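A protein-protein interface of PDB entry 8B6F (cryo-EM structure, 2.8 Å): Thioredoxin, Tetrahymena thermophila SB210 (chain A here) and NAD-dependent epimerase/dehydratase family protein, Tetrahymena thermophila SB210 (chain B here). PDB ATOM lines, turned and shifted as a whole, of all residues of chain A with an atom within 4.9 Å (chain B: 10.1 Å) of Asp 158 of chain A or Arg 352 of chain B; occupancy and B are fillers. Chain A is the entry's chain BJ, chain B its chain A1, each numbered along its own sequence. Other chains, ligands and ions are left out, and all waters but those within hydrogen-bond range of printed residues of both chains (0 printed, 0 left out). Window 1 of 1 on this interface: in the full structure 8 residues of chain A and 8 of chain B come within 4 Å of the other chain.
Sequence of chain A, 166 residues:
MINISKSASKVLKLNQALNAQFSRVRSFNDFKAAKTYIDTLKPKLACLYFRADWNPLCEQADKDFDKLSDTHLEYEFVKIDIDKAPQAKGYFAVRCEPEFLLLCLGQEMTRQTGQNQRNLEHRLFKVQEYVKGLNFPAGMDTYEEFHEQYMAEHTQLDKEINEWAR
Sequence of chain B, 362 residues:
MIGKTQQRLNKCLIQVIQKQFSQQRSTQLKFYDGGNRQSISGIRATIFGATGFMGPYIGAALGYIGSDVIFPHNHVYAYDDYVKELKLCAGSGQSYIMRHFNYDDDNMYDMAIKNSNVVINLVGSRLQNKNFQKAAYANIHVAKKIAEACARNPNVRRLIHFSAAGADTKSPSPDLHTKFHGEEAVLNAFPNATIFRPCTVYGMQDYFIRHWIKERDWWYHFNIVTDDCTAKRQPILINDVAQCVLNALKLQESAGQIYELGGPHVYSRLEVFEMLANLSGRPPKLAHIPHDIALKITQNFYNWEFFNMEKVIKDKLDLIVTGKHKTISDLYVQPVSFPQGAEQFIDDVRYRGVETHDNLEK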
ATOM      1  N   GLU A 153     -31.894 -17.916  34.246  1.00  0.00           N
ATOM      2  CA  GLU A 153     -30.707 -17.941  33.398  1.00  0.00           C
ATOM      3  C   GLU A 153     -30.553 -16.632  32.636  1.00  0.00           C
ATOM      4  O   GLU A 153     -29.435 -16.150  32.430  1.00  0.00           O
ATOM      5  CB  GLU A 153     -30.774 -19.120  32.429  1.00  0.00           C
ATOM      6  CG  GLU A 153     -30.727 -20.473  33.112  1.00  0.00           C
ATOM      7  CD  GLU A 153     -30.786 -21.621  32.128  1.00  0.00           C
ATOM      8  OE1 GLU A 153     -30.870 -21.354  30.912  1.00  0.00           O
ATOM      9  OE2 GLU A 153     -30.750 -22.787  32.570  1.00  0.00           O
ATOM     10  N   HIS A 154     -31.673 -16.044  32.212  1.00  0.00           N
ATOM     11  CA  HIS A 154     -31.626 -14.760  31.522  1.00  0.00           C
ATOM     12  C   HIS A 154     -31.024 -13.687  32.418  1.00  0.00           C
ATOM     13  O   HIS A 154     -30.085 -12.988  32.026  1.00  0.00           O
ATOM     14  CB  HIS A 154     -33.033 -14.367  31.070  1.00  0.00           C
ATOM     15  CG  HIS A 154     -33.090 -13.088  30.295  1.00  0.00           C
ATOM     16  ND1 HIS A 154     -33.020 -11.850  30.896  1.00  0.00           N
ATOM     17  CD2 HIS A 154     -33.228 -12.854  28.968  1.00  0.00           C
ATOM     18  CE1 HIS A 154     -33.103 -10.910  29.972  1.00  0.00           C
ATOM     19  NE2 HIS A 154     -33.231 -11.492  28.794  1.00  0.00           N
ATOM     20  N   GLN A 156     -29.128 -14.097  34.848  1.00  0.00           N
ATOM     21  CA  GLN A 156     -27.744 -14.417  35.177  1.00  0.00           C
ATOM     22  C   GLN A 156     -26.792 -14.052  34.043  1.00  0.00           C
ATOM     23  O   GLN A 156     -25.700 -13.528  34.291  1.00  0.00           O
ATOM     24  CB  GLN A 156     -27.619 -15.900  35.521  1.00  0.00           C
ATOM     25  CG  GLN A 156     -26.261 -16.280  36.076  1.00  0.00           C
ATOM     26  CD  GLN A 156     -26.246 -17.673  36.661  1.00  0.00           C
ATOM     27  OE1 GLN A 156     -27.204 -18.431  36.517  1.00  0.00           O
ATOM     28  NE2 GLN A 156     -25.154 -18.019  37.332  1.00  0.00           N
ATOM     29  N   LEU A 157     -27.179 -14.321  32.795  1.00  0.00           N
ATOM     30  CA  LEU A 157     -26.279 -14.174  31.656  1.00  0.00           C
ATOM     31  C   LEU A 157     -26.711 -13.070  30.701  1.00  0.00           C
ATOM     32  O   LEU A 157     -25.939 -12.147  30.434  1.00  0.00           O
ATOM     33  CB  LEU A 157     -26.175 -15.503  30.897  1.00  0.00           C
ATOM     34  CG  LEU A 157     -25.670 -16.710  31.685  1.00  0.00           C
ATOM     35  CD1 LEU A 157     -25.759 -17.958  30.830  1.00  0.00           C
ATOM     36  CD2 LEU A 157     -24.248 -16.490  32.173  1.00  0.00           C
ATOM     37  N   ASP A 158     -27.937 -13.136  30.182  1.00  0.00           N
ATOM     38  CA  ASP A 158     -28.326 -12.229  29.108  1.00  0.00           C
ATOM     39  C   ASP A 158     -28.450 -10.797  29.607  1.00  0.00           C
ATOM     40  O   ASP A 158     -28.100  -9.853  28.890  1.00  0.00           O
ATOM     41  CB  ASP A 158     -29.643 -12.688  28.486  1.00  0.00           C
ATOM     42  CG  ASP A 158     -29.597 -14.126  28.025  1.00  0.00           C
ATOM     43  OD1 ASP A 158     -29.315 -15.006  28.864  1.00  0.00           O
ATOM     44  OD2 ASP A 158     -29.847 -14.379  26.829  1.00  0.00           O
ATOM     45  N   LYS A 159     -28.945 -10.612  30.830  1.00  0.00           N
ATOM     46  CA  LYS A 159     -29.070  -9.262  31.364  1.00  0.00           C
ATOM     47  C   LYS A 159     -27.710  -8.594  31.490  1.00  0.00           C
ATOM     48  O   LYS A 159     -27.547  -7.428  31.117  1.00  0.00           O
ATOM     49  CB  LYS A 159     -29.790  -9.287  32.711  1.00  0.00           C
ATOM     50  CG  LYS A 159     -30.265  -7.914  33.160  1.00  0.00           C
ATOM     51  CD  LYS A 159     -30.958  -7.953  34.511  1.00  0.00           C
ATOM     52  CE  LYS A 159     -29.968  -8.183  35.636  1.00  0.00           C
ATOM     53  NZ  LYS A 159     -30.614  -8.076  36.974  1.00  0.00           N
ATOM     54  N   GLU A 160     -26.717  -9.317  32.005  1.00  0.00           N
ATOM     55  CA  GLU A 160     -25.377  -8.751  32.099  1.00  0.00           C
ATOM     56  C   GLU A 160     -24.791  -8.487  30.717  1.00  0.00           C
ATOM     57  O   GLU A 160     -24.135  -7.462  30.504  1.00  0.00           O
ATOM     58  CB  GLU A 160     -24.477  -9.684  32.905  1.00  0.00           C
ATOM     59  CG  GLU A 160     -24.865  -9.763  34.373  1.00  0.00           C
ATOM     60  CD  GLU A 160     -23.940 -10.651  35.177  1.00  0.00           C
ATOM     61  OE1 GLU A 160     -23.263 -11.508  34.571  1.00  0.00           O
ATOM     62  OE2 GLU A 160     -23.885 -10.489  36.413  1.00  0.00           O
ATOM     63  N   ILE A 161     -25.010  -9.399  29.767  1.00  0.00           N
ATOM     64  CA  ILE A 161     -24.493  -9.192  28.417  1.00  0.00           C
ATOM     65  C   ILE A 161     -25.096  -7.934  27.806  1.00  0.00           C
ATOM     66  O   ILE A 161     -24.395  -7.134  27.175  1.00  0.00           O
ATOM     67  CB  ILE A 161     -24.757 -10.433  27.543  1.00  0.00           C
ATOM     68  CG1 ILE A 161     -23.872 -11.594  28.003  1.00  0.00           C
ATOM     69  CG2 ILE A 161     -24.499 -10.122  26.072  1.00  0.00           C
ATOM     70  CD1 ILE A 161     -24.193 -12.919  27.345  1.00  0.00           C
ATOM     71  N   ASN A 162     -26.403  -7.737  27.981  1.00  0.00           N
ATOM     72  CA  ASN A 162     -27.041  -6.531  27.464  1.00  0.00           C
ATOM     73  C   ASN A 162     -26.526  -5.287  28.171  1.00  0.00           C
ATOM     74  O   ASN A 162     -26.276  -4.260  27.528  1.00  0.00           O
ATOM     75  CB  ASN A 162     -28.559  -6.633  27.610  1.00  0.00           C
ATOM     76  CG  ASN A 162     -29.269  -5.377  27.148  1.00  0.00           C
ATOM     77  OD1 ASN A 162     -29.545  -5.206  25.962  1.00  0.00           O
ATOM     78  ND2 ASN A 162     -29.567  -4.487  28.086  1.00  0.00           N
ATOM     79  N   GLU A 163     -26.368  -5.351  29.492  1.00  0.00           N
ATOM     80  CA  GLU A 163     -25.877  -4.195  30.231  1.00  0.00           C
ATOM     81  C   GLU A 163     -24.455  -3.835  29.831  1.00  0.00           C
ATOM     82  O   GLU A 163     -24.050  -2.675  29.966  1.00  0.00           O
ATOM     83  CB  GLU A 163     -25.957  -4.463  31.733  1.00  0.00           C
ATOM     84  CG  GLU A 163     -27.383  -4.515  32.254  1.00  0.00           C
ATOM     85  CD  GLU A 163     -27.472  -4.950  33.701  1.00  0.00           C
ATOM     86  OE1 GLU A 163     -26.464  -5.447  34.241  1.00  0.00           O
ATOM     87  OE2 GLU A 163     -28.557  -4.797  34.300  1.00  0.00           O
ATOM     88  N   ALA A 165     -23.093  -4.611  26.541  1.00  0.00           N
ATOM     89  CA  ALA A 165     -23.191  -4.206  25.145  1.00  0.00           C
ATOM     90  C   ALA A 165     -24.617  -3.758  24.863  1.00  0.00           C
ATOM     91  O   ALA A 165     -25.557  -4.545  25.004  1.00  0.00           O
ATOM     92  CB  ALA A 165     -22.799  -5.355  24.217  1.00  0.00           C
ATOM     93  N   ARG A 166     -24.769  -2.503  24.453  1.00  0.00           N
ATOM     94  CA  ARG A 166     -26.081  -1.942  24.156  1.00  0.00           C
ATOM     95  C   ARG A 166     -27.043  -2.153  25.320  1.00  0.00           C
ATOM     96  O   ARG A 166     -26.871  -1.570  26.390  1.00  0.00           O
ATOM     97  CB  ARG A 166     -26.653  -2.561  22.879  1.00  0.00           C
ATOM     98  CG  ARG A 166     -28.085  -2.148  22.587  1.00  0.00           C
ATOM     99  CD  ARG A 166     -28.471  -2.436  21.145  1.00  0.00           C
ATOM    100  NE  ARG A 166     -28.302  -3.840  20.791  1.00  0.00           N
ATOM    101  CZ  ARG A 166     -27.215  -4.357  20.234  1.00  0.00           C
ATOM    102  NH1 ARG A 166     -26.156  -3.614  19.955  1.00  0.00           N
ATOM    103  NH2 ARG A 166     -27.189  -5.655  19.946  1.00  0.00           N
ATOM    104  N   TYR B 220     -35.197   3.112  32.280  1.00  0.00           N
ATOM    105  CA  TYR B 220     -34.273   1.982  32.275  1.00  0.00           C
ATOM    106  C   TYR B 220     -34.737   0.846  33.178  1.00  0.00           C
ATOM    107  O   TYR B 220     -34.149  -0.240  33.165  1.00  0.00           O
ATOM    108  CB  TYR B 220     -32.866   2.416  32.688  1.00  0.00           C
ATOM    109  CG  TYR B 220     -31.853   1.314  32.502  1.00  0.00           C
ATOM    110  CD1 TYR B 220     -31.322   1.034  31.250  1.00  0.00           C
ATOM    111  CD2 TYR B 220     -31.449   0.535  33.576  1.00  0.00           C
ATOM    112  CE1 TYR B 220     -30.409   0.017  31.078  1.00  0.00           C
ATOM    113  CE2 TYR B 220     -30.538  -0.482  33.415  1.00  0.00           C
ATOM    114  CZ  TYR B 220     -30.021  -0.735  32.165  1.00  0.00           C
ATOM    115  OH  TYR B 220     -29.113  -1.749  32.007  1.00  0.00           O
ATOM    116  N   LEU B 279     -41.530  -8.691  20.971  1.00  0.00           N
ATOM    117  CA  LEU B 279     -40.902  -8.389  19.691  1.00  0.00           C
ATOM    118  C   LEU B 279     -39.490  -7.847  19.876  1.00  0.00           C
ATOM    119  O   LEU B 279     -38.567  -8.255  19.162  1.00  0.00           O
ATOM    120  CB  LEU B 279     -41.759  -7.396  18.909  1.00  0.00           C
ATOM    121  CG  LEU B 279     -43.113  -7.890  18.395  1.00  0.00           C
ATOM    122  CD1 LEU B 279     -43.853  -6.757  17.711  1.00  0.00           C
ATOM    123  CD2 LEU B 279     -42.942  -9.058  17.441  1.00  0.00           C
ATOM    124  N   SER B 280     -39.299  -6.926  20.821  1.00  0.00           N
ATOM    125  CA  SER B 280     -38.010  -6.270  20.996  1.00  0.00           C
ATOM    126  C   SER B 280     -37.046  -7.057  21.870  1.00  0.00           C
ATOM    127  O   SER B 280     -35.850  -6.752  21.871  1.00  0.00           O
ATOM    128  CB  SER B 280     -38.190  -4.886  21.623  1.00  0.00           C
ATOM    129  OG  SER B 280     -38.792  -4.998  22.897  1.00  0.00           O
ATOM    130  N   GLY B 281     -37.526  -8.055  22.609  1.00  0.00           N
ATOM    131  CA  GLY B 281     -36.683  -8.794  23.520  1.00  0.00           C
ATOM    132  C   GLY B 281     -36.504  -8.156  24.880  1.00  0.00           C
ATOM    133  O   GLY B 281     -35.909  -8.785  25.764  1.00  0.00           O
ATOM    134  N   ARG B 282     -36.992  -6.938  25.081  1.00  0.00           N
ATOM    135  CA  ARG B 282     -36.832  -6.260  26.361  1.00  0.00           C
ATOM    136  C   ARG B 282     -37.822  -6.823  27.374  1.00  0.00           C
ATOM    137  O   ARG B 282     -39.027  -6.833  27.108  1.00  0.00           O
ATOM    138  CB  ARG B 282     -37.058  -4.760  26.206  1.00  0.00           C
ATOM    139  CG  ARG B 282     -35.993  -4.043  25.398  1.00  0.00           C
ATOM    140  CD  ARG B 282     -36.259  -2.547  25.363  1.00  0.00           C
ATOM    141  NE  ARG B 282     -35.167  -1.810  24.740  1.00  0.00           N
ATOM    142  CZ  ARG B 282     -35.112  -0.488  24.645  1.00  0.00           C
ATOM    143  NH1 ARG B 282     -36.078   0.280  25.122  1.00  0.00           N
ATOM    144  NH2 ARG B 282     -34.061   0.078  24.060  1.00  0.00           N
ATOM    145  N   PRO B 283     -37.365  -7.291  28.533  1.00  0.00           N
ATOM    146  CA  PRO B 283     -38.303  -7.781  29.545  1.00  0.00           C
ATOM    147  C   PRO B 283     -39.282  -6.692  29.943  1.00  0.00           C
ATOM    148  O   PRO B 283     -38.898  -5.518  30.056  1.00  0.00           O
ATOM    149  CB  PRO B 283     -37.390  -8.166  30.719  1.00  0.00           C
ATOM    150  CG  PRO B 283     -36.072  -8.426  30.104  1.00  0.00           C
ATOM    151  CD  PRO B 283     -35.966  -7.472  28.955  1.00  0.00           C
ATOM    152  N   ILE B 346     -38.502  -1.454  15.667  1.00  0.00           N
ATOM    153  CA  ILE B 346     -37.801  -1.751  16.908  1.00  0.00           C
ATOM    154  C   ILE B 346     -36.555  -2.600  16.659  1.00  0.00           C
ATOM    155  O   ILE B 346     -36.026  -3.205  17.581  1.00  0.00           O
ATOM    156  CB  ILE B 346     -38.742  -2.427  17.921  1.00  0.00           C
ATOM    157  CG1 ILE B 346     -39.218  -3.770  17.369  1.00  0.00           C
ATOM    158  CG2 ILE B 346     -39.918  -1.514  18.232  1.00  0.00           C
ATOM    159  CD1 ILE B 346     -40.136  -4.522  18.282  1.00  0.00           C
ATOM    160  N   ASP B 347     -36.082  -2.656  15.413  1.00  0.00           N
ATOM    161  CA  ASP B 347     -34.902  -3.458  15.104  1.00  0.00           C
ATOM    162  C   ASP B 347     -33.676  -2.936  15.844  1.00  0.00           C
ATOM    163  O   ASP B 347     -32.904  -3.712  16.418  1.00  0.00           O
ATOM    164  CB  ASP B 347     -34.658  -3.465  13.596  1.00  0.00           C
ATOM    165  CG  ASP B 347     -33.454  -4.300  13.204  1.00  0.00           C
ATOM    166  OD1 ASP B 347     -33.533  -5.542  13.300  1.00  0.00           O
ATOM    167  OD2 ASP B 347     -32.428  -3.713  12.802  1.00  0.00           O
ATOM    168  N   ASP B 348     -33.478  -1.616  15.839  1.00  0.00           N
ATOM    169  CA  ASP B 348     -32.318  -1.048  16.519  1.00  0.00           C
ATOM    170  C   ASP B 348     -32.390  -1.288  18.020  1.00  0.00           C
ATOM    171  O   ASP B 348     -31.384  -1.640  18.648  1.00  0.00           O
ATOM    172  CB  ASP B 348     -32.212   0.447  16.222  1.00  0.00           C
ATOM    173  CG  ASP B 348     -31.724   0.729  14.813  1.00  0.00           C
ATOM    174  OD1 ASP B 348     -31.368  -0.234  14.100  1.00  0.00           O
ATOM    175  OD2 ASP B 348     -31.693   1.914  14.419  1.00  0.00           O
ATOM    176  N   VAL B 349     -33.565  -1.103  18.613  1.00  0.00           N
ATOM    177  CA  VAL B 349     -33.735  -1.301  20.062  1.00  0.00           C
ATOM    178  C   VAL B 349     -34.125  -2.763  20.249  1.00  0.00           C
ATOM    179  O   VAL B 349     -35.294  -3.136  20.356  1.00  0.00           O
ATOM    180  CB  VAL B 349     -34.744  -0.316  20.666  1.00  0.00           C
ATOM    181  CG1 VAL B 349     -34.269   1.107  20.452  1.00  0.00           C
ATOM    182  CG2 VAL B 349     -36.138  -0.473  20.055  1.00  0.00           C
ATOM    183  N   ARG B 350     -33.109  -3.618  20.293  1.00  0.00           N
ATOM    184  CA  ARG B 350     -33.293  -5.040  20.537  1.00  0.00           C
ATOM    185  C   ARG B 350     -32.401  -5.467  21.688  1.00  0.00           C
ATOM    186  O   ARG B 350     -31.238  -5.065  21.766  1.00  0.00           O
ATOM    187  CB  ARG B 350     -32.970  -5.877  19.297  1.00  0.00           C
ATOM    188  CG  ARG B 350     -34.129  -6.009  18.333  1.00  0.00           C
ATOM    189  CD  ARG B 350     -33.806  -6.974  17.206  1.00  0.00           C
ATOM    190  NE  ARG B 350     -34.974  -7.232  16.373  1.00  0.00           N
ATOM    191  CZ  ARG B 350     -34.979  -8.017  15.305  1.00  0.00           C
ATOM    192  NH1 ARG B 350     -33.885  -8.641  14.901  1.00  0.00           N
ATOM    193  NH2 ARG B 350     -36.109  -8.176  14.622  1.00  0.00           N
ATOM    194  N   TYR B 351     -32.958  -6.278  22.580  1.00  0.00           N
ATOM    195  CA  TYR B 351     -32.188  -6.780  23.706  1.00  0.00           C
ATOM    196  C   TYR B 351     -31.014  -7.604  23.199  1.00  0.00           C
ATOM    197  O   TYR B 351     -31.171  -8.452  22.317  1.00  0.00           O
ATOM    198  CB  TYR B 351     -33.083  -7.618  24.611  1.00  0.00           C
ATOM    199  CG  TYR B 351     -32.683  -7.585  26.061  1.00  0.00           C
ATOM    200  CD1 TYR B 351     -33.076  -6.531  26.870  1.00  0.00           C
ATOM    201  CD2 TYR B 351     -31.933  -8.605  26.626  1.00  0.00           C
ATOM    202  CE1 TYR B 351     -32.730  -6.484  28.194  1.00  0.00           C
ATOM    203  CE2 TYR B 351     -31.579  -8.568  27.957  1.00  0.00           C
ATOM    204  CZ  TYR B 351     -31.989  -7.502  28.736  1.00  0.00           C
ATOM    205  OH  TYR B 351     -31.651  -7.438  30.062  1.00  0.00           O
ATOM    206  N   ARG B 352     -29.835  -7.346  23.750  1.00  0.00           N
ATOM    207  CA  ARG B 352     -28.611  -8.036  23.357  1.00  0.00           C
ATOM    208  C   ARG B 352     -28.269  -9.033  24.460  1.00  0.00           C
ATOM    209  O   ARG B 352     -27.562  -8.707  25.415  1.00  0.00           O
ATOM    210  CB  ARG B 352     -27.474  -7.045  23.117  1.00  0.00           C
ATOM    211  CG  ARG B 352     -26.147  -7.692  22.743  1.00  0.00           C
ATOM    212  CD  ARG B 352     -26.284  -8.577  21.515  1.00  0.00           C
ATOM    213  NE  ARG B 352     -24.992  -9.042  21.023  1.00  0.00           N
ATOM    214  CZ  ARG B 352     -24.371 -10.137  21.441  1.00  0.00           C
ATOM    215  NH1 ARG B 352     -24.888 -10.911  22.380  1.00  0.00           N
ATOM    216  NH2 ARG B 352     -23.204 -10.467  20.898  1.00  0.00           N
ATOM    217  N   GLY B 353     -28.777 -10.247  24.323  1.00  0.00           N
ATOM    218  CA  GLY B 353     -28.488 -11.335  25.238  1.00  0.00           C
ATOM    219  C   GLY B 353     -27.455 -12.284  24.670  1.00  0.00           C
ATOM    220  O   GLY B 353     -26.470 -11.865  24.051  1.00  0.00           O
ATOM    221  N   VAL B 354     -27.682 -13.576  24.877  1.00  0.00           N
ATOM    222  CA  VAL B 354     -26.804 -14.605  24.331  1.00  0.00           C
ATOM    223  C   VAL B 354     -27.147 -14.791  22.860  1.00  0.00           C
ATOM    224  O   VAL B 354     -28.299 -15.070  22.512  1.00  0.00           O
ATOM    225  CB  VAL B 354     -26.946 -15.923  25.106  1.00  0.00           C
ATOM    226  CG1 VAL B 354     -26.066 -17.000  24.491  1.00  0.00           C
ATOM    227  CG2 VAL B 354     -26.592 -15.718  26.569  1.00  0.00           C
ATOM    228  N   GLU B 355     -26.150 -14.633  21.995  1.00  0.00           N
ATOM    229  CA  GLU B 355     -26.349 -14.727  20.558  1.00  0.00           C
ATOM    230  C   GLU B 355     -25.207 -15.523  19.944  1.00  0.00           C
ATOM    231  O   GLU B 355     -24.127 -15.652  20.525  1.00  0.00           O
ATOM    232  CB  GLU B 355     -26.443 -13.339  19.914  1.00  0.00           C
ATOM    233  CG  GLU B 355     -27.639 -12.533  20.392  1.00  0.00           C
ATOM    234  CD  GLU B 355     -27.687 -11.148  19.788  1.00  0.00           C
ATOM    235  OE1 GLU B 355     -26.659 -10.707  19.234  1.00  0.00           O
ATOM    236  OE2 GLU B 355     -28.752 -10.499  19.865  1.00  0.00           O
ATOM    237  N   THR B 356     -25.465 -16.059  18.757  1.00  0.00           N
ATOM    238  CA  THR B 356     -24.489 -16.892  18.075  1.00  0.00           C
ATOM    239  C   THR B 356     -23.322 -16.048  17.572  1.00  0.00           C
ATOM    240  O   THR B 356     -23.429 -14.835  17.380  1.00  0.00           O
ATOM    241  CB  THR B 356     -25.138 -17.629  16.903  1.00  0.00           C
ATOM    242  OG1 THR B 356     -25.663 -16.680  15.966  1.00  0.00           O
ATOM    243  CG2 THR B 356     -26.263 -18.526  17.391  1.00  0.00           C
ATOM    244  N   HIS B 357     -22.186 -16.716  17.363  1.00  0.00           N
ATOM    245  CA  HIS B 357     -21.015 -16.030  16.828  1.00  0.00           C
ATOM    246  C   HIS B 357     -21.294 -15.480  15.437  1.00  0.00           C
ATOM    247  O   HIS B 357     -20.823 -14.394  15.082  1.00  0.00           O
ATOM    248  CB  HIS B 357     -19.816 -16.975  16.801  1.00  0.00           C
ATOM    249  CG  HIS B 357     -18.551 -16.327  16.332  1.00  0.00           C
ATOM    250  ND1 HIS B 357     -18.095 -16.433  15.036  1.00  0.00           N
ATOM    251  CD2 HIS B 357     -17.651 -15.554  16.985  1.00  0.00           C
ATOM    252  CE1 HIS B 357     -16.968 -15.758  14.912  1.00  0.00           C
ATOM    253  NE2 HIS B 357     -16.676 -15.214  16.080  1.00  0.00           N
ATOM    254  N   ASP B 358     -22.055 -16.219  14.628  1.00  0.00           N
ATOM    255  CA  ASP B 358     -22.458 -15.704  13.326  1.00  0.00           C
ATOM    256  C   ASP B 358     -23.286 -14.435  13.476  1.00  0.00           C
ATOM    257  O   ASP B 358     -23.093 -13.465  12.736  1.00  0.00           O
ATOM    258  CB  ASP B 358     -23.242 -16.768  12.558  1.00  0.00           C
ATOM    259  CG  ASP B 358     -22.430 -18.023  12.310  1.00  0.00           C
ATOM    260  OD1 ASP B 358     -21.260 -18.073  12.743  1.00  0.00           O
ATOM    261  OD2 ASP B 358     -22.960 -18.959  11.675  1.00  0.00           O
ATOM    262  N   ASN B 359     -24.214 -14.424  14.434  1.00  0.00           N
ATOM    263  CA  ASN B 359     -24.999 -13.226  14.700  1.00  0.00           C
ATOM    264  C   ASN B 359     -24.142 -12.080  15.217  1.00  0.00           C
ATOM    265  O   ASN B 359     -24.540 -10.918  15.087  1.00  0.00           O
ATOM    266  CB  ASN B 359     -26.106 -13.541  15.707  1.00  0.00           C
ATOM    267  CG  ASN B 359     -27.033 -12.369  15.933  1.00  0.00           C
ATOM    268  OD1 ASN B 359     -26.731 -11.465  16.709  1.00  0.00           O
ATOM    269  ND2 ASN B 359     -28.173 -12.380  15.256  1.00  0.00           N
ATOM    270  N   LEU B 360     -22.985 -12.378  15.810  1.00  0.00           N
ATOM    271  CA  LEU B 360     -22.097 -11.324  16.285  1.00  0.00           C
ATOM    272  C   LEU B 360     -21.549 -10.476  15.147  1.00  0.00           C
ATOM    273  O   LEU B 360     -21.112  -9.345  15.387  1.00  0.00           O
ATOM    274  CB  LEU B 360     -20.939 -11.935  17.079  1.00  0.00           C
ATOM    275  CG  LEU B 360     -19.848 -10.975  17.555  1.00  0.00           C
ATOM    276  CD1 LEU B 360     -20.423  -9.915  18.475  1.00  0.00           C
ATOM    277  CD2 LEU B 360     -18.740 -11.738  18.251  1.00  0.00           C
ATOM    278  N   GLU B 361     -21.555 -10.991  13.917  1.00  0.00           N
ATOM    279  CA  GLU B 361     -20.966 -10.248  12.809  1.00  0.00           C
ATOM    280  C   GLU B 361     -21.700  -8.935  12.569  1.00  0.00           C
ATOM    281  O   GLU B 361     -21.069  -7.895  12.354  1.00  0.00           O
ATOM    282  CB  GLU B 361     -20.974 -11.104  11.542  1.00  0.00           C
ATOM    283  CG  GLU B 361     -20.437 -10.391  10.312  1.00  0.00           C
ATOM    284  CD  GLU B 361     -19.050  -9.819  10.530  1.00  0.00           C
ATOM    285  OE1 GLU B 361     -18.304 -10.369  11.367  1.00  0.00           O
ATOM    286  OE2 GLU B 361     -18.707  -8.814   9.872  1.00  0.00           O
ATOM    287  N   LYS B 362     -23.026  -8.963  12.598  1.00  0.00           N
ATOM    288  CA  LYS B 362     -23.820  -7.755  12.406  1.00  0.00           C
ATOM    289  C   LYS B 362     -23.566  -7.153  11.030  1.00  0.00           C
ATOM    290  O   LYS B 362     -24.203  -6.174  10.636  1.00  0.00           O
ATOM    291  CB  LYS B 362     -23.503  -6.728  13.495  1.00  0.00           C
ATOM    292  CG  LYS B 362     -24.622  -5.732  13.748  1.00  0.00           C
ATOM    293  CD  LYS B 362     -25.743  -6.357  14.564  1.00  0.00           C
ATOM    294  CE  LYS B 362     -26.809  -5.330  14.916  1.00  0.00           C
ATOM    295  NZ  LYS B 362     -27.906  -5.923  15.732  1.00  0.00           N
ATOM    296  OXT LYS B 362     -22.713  -7.620  10.280  1.00  0.00           O
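Of chain B, only Tyr 351, Arg 352, Gly 353 and Val 354 come within 4 Å of Asp 158 of chain A.
Arg 352 of chain B touches just these residues of chain A: Asp 158, Ile 161, Asn 162, Ala 165 and Arg 166.
His 154 of chain A touches just these residues of chain B: Pro 283 and Tyr 351.
Of the printed residues of chain B, Ile 161 of chain A touches Arg 352 (3.4 Å), Gly 353 (3.3 Å) and Val 354 (3.8 Å).
Of the printed residues of chain B, Asn 162 of chain A touches Tyr 351 and Arg 352.
Of chain B, only Arg 352 comes within 4 Å of Ala 165 of chain A.
Printed residues of chain A within 4 Å of Gly 353 of chain B: Asp 158 (3.7 Å) and Ile 161 (3.3 Å).
Printed residues of chain A within 4 Å of Asp 348 of chain B: Arg 166 (3.9 Å).
Of the printed residues of chain A, Arg 350 of chain B touches Arg 166.
Of the printed residues of chain B, Arg 166 of chain A touches Asp 348, Arg 350 and Arg 352.
Of the printed residues of chain B, Lys 159 of chain A touches Tyr 351.
Thr 356 of chain B touches none of the printed residues of chain A.
Arg 282 of chain B touches none of the printed residues of chain A.
The nearest printed residue of chain A that does not touch Tyr 220 of chain B is Asn 162 of chain A (4.8 Å).
Printed residues of chain B that touch a printed residue of chain A: Tyr 220, Pro 283, Asp 348, Arg 350, Tyr 351, Arg 352, Gly 353 and Val 354.
Among the printed residues, no Asp or Glu carboxylate lies within 4 Å of a Lys or Arg side-chain nitrogen of the other chain.
O of Ser 280 of chain B is in hydrogen-bond range of N of Tyr 351 of chain B, at 3.0 Å.
The guanidinium group of Arg 350 of chain B lies within salt-bridge range of the side-chain carboxylate of Asp 347 of chain B (3.5 Å).
The side-chain carboxylate of Glu 355 of chain B is in salt-bridge range of the guanidinium group of Arg 352 of chain B, 3.0 Å away.
O of His 154 of chain A sits at hydrogen-bond distance from N of Lys 159 of chain A (2.9 Å).
NE of Arg 166 of chain A is in hydrogen-bond range of O of Arg 350 of chain B (3.3 Å).
The backbone carbonyl oxygen (O) of Arg 352 of chain B is in hydrogen-bond range of the backbone NH (N) of Asn 162 of chain A, 3.0 Å away.
N of Val 354 of chain B lies within hydrogen-bond range of OD2 of Asp 158 of chain A, at 3.0 Å.
Tyr 351 of chain B touches His 154 of chain A (CE2 to CE1, 3.4 Å).
Asp 158 of chain A touches Tyr 351 of chain B (O to CE2, 3.8 Å).
Asp 158 of chain A touches Arg 352 of chain B.
CA of Gly 353 of chain B touches OD2 of Asp 158 of chain A (3.7 Å).
Lys 159 of chain A touches Tyr 351 of chain B (CA to OH, 3.4 Å).
Ile 161 of chain A touches Gly 353 of chain B (CG2 to O, 3.3 Å).
Ile 161 of chain A touches Val 354 of chain B.
Asn 162 of chain A touches Tyr 351 of chain B.
Glu 163 of chain A touches Tyr 220 of chain B.
Arg 166 of chain A touches Asp 348 of chain B (CD to O, 3.9 Å).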
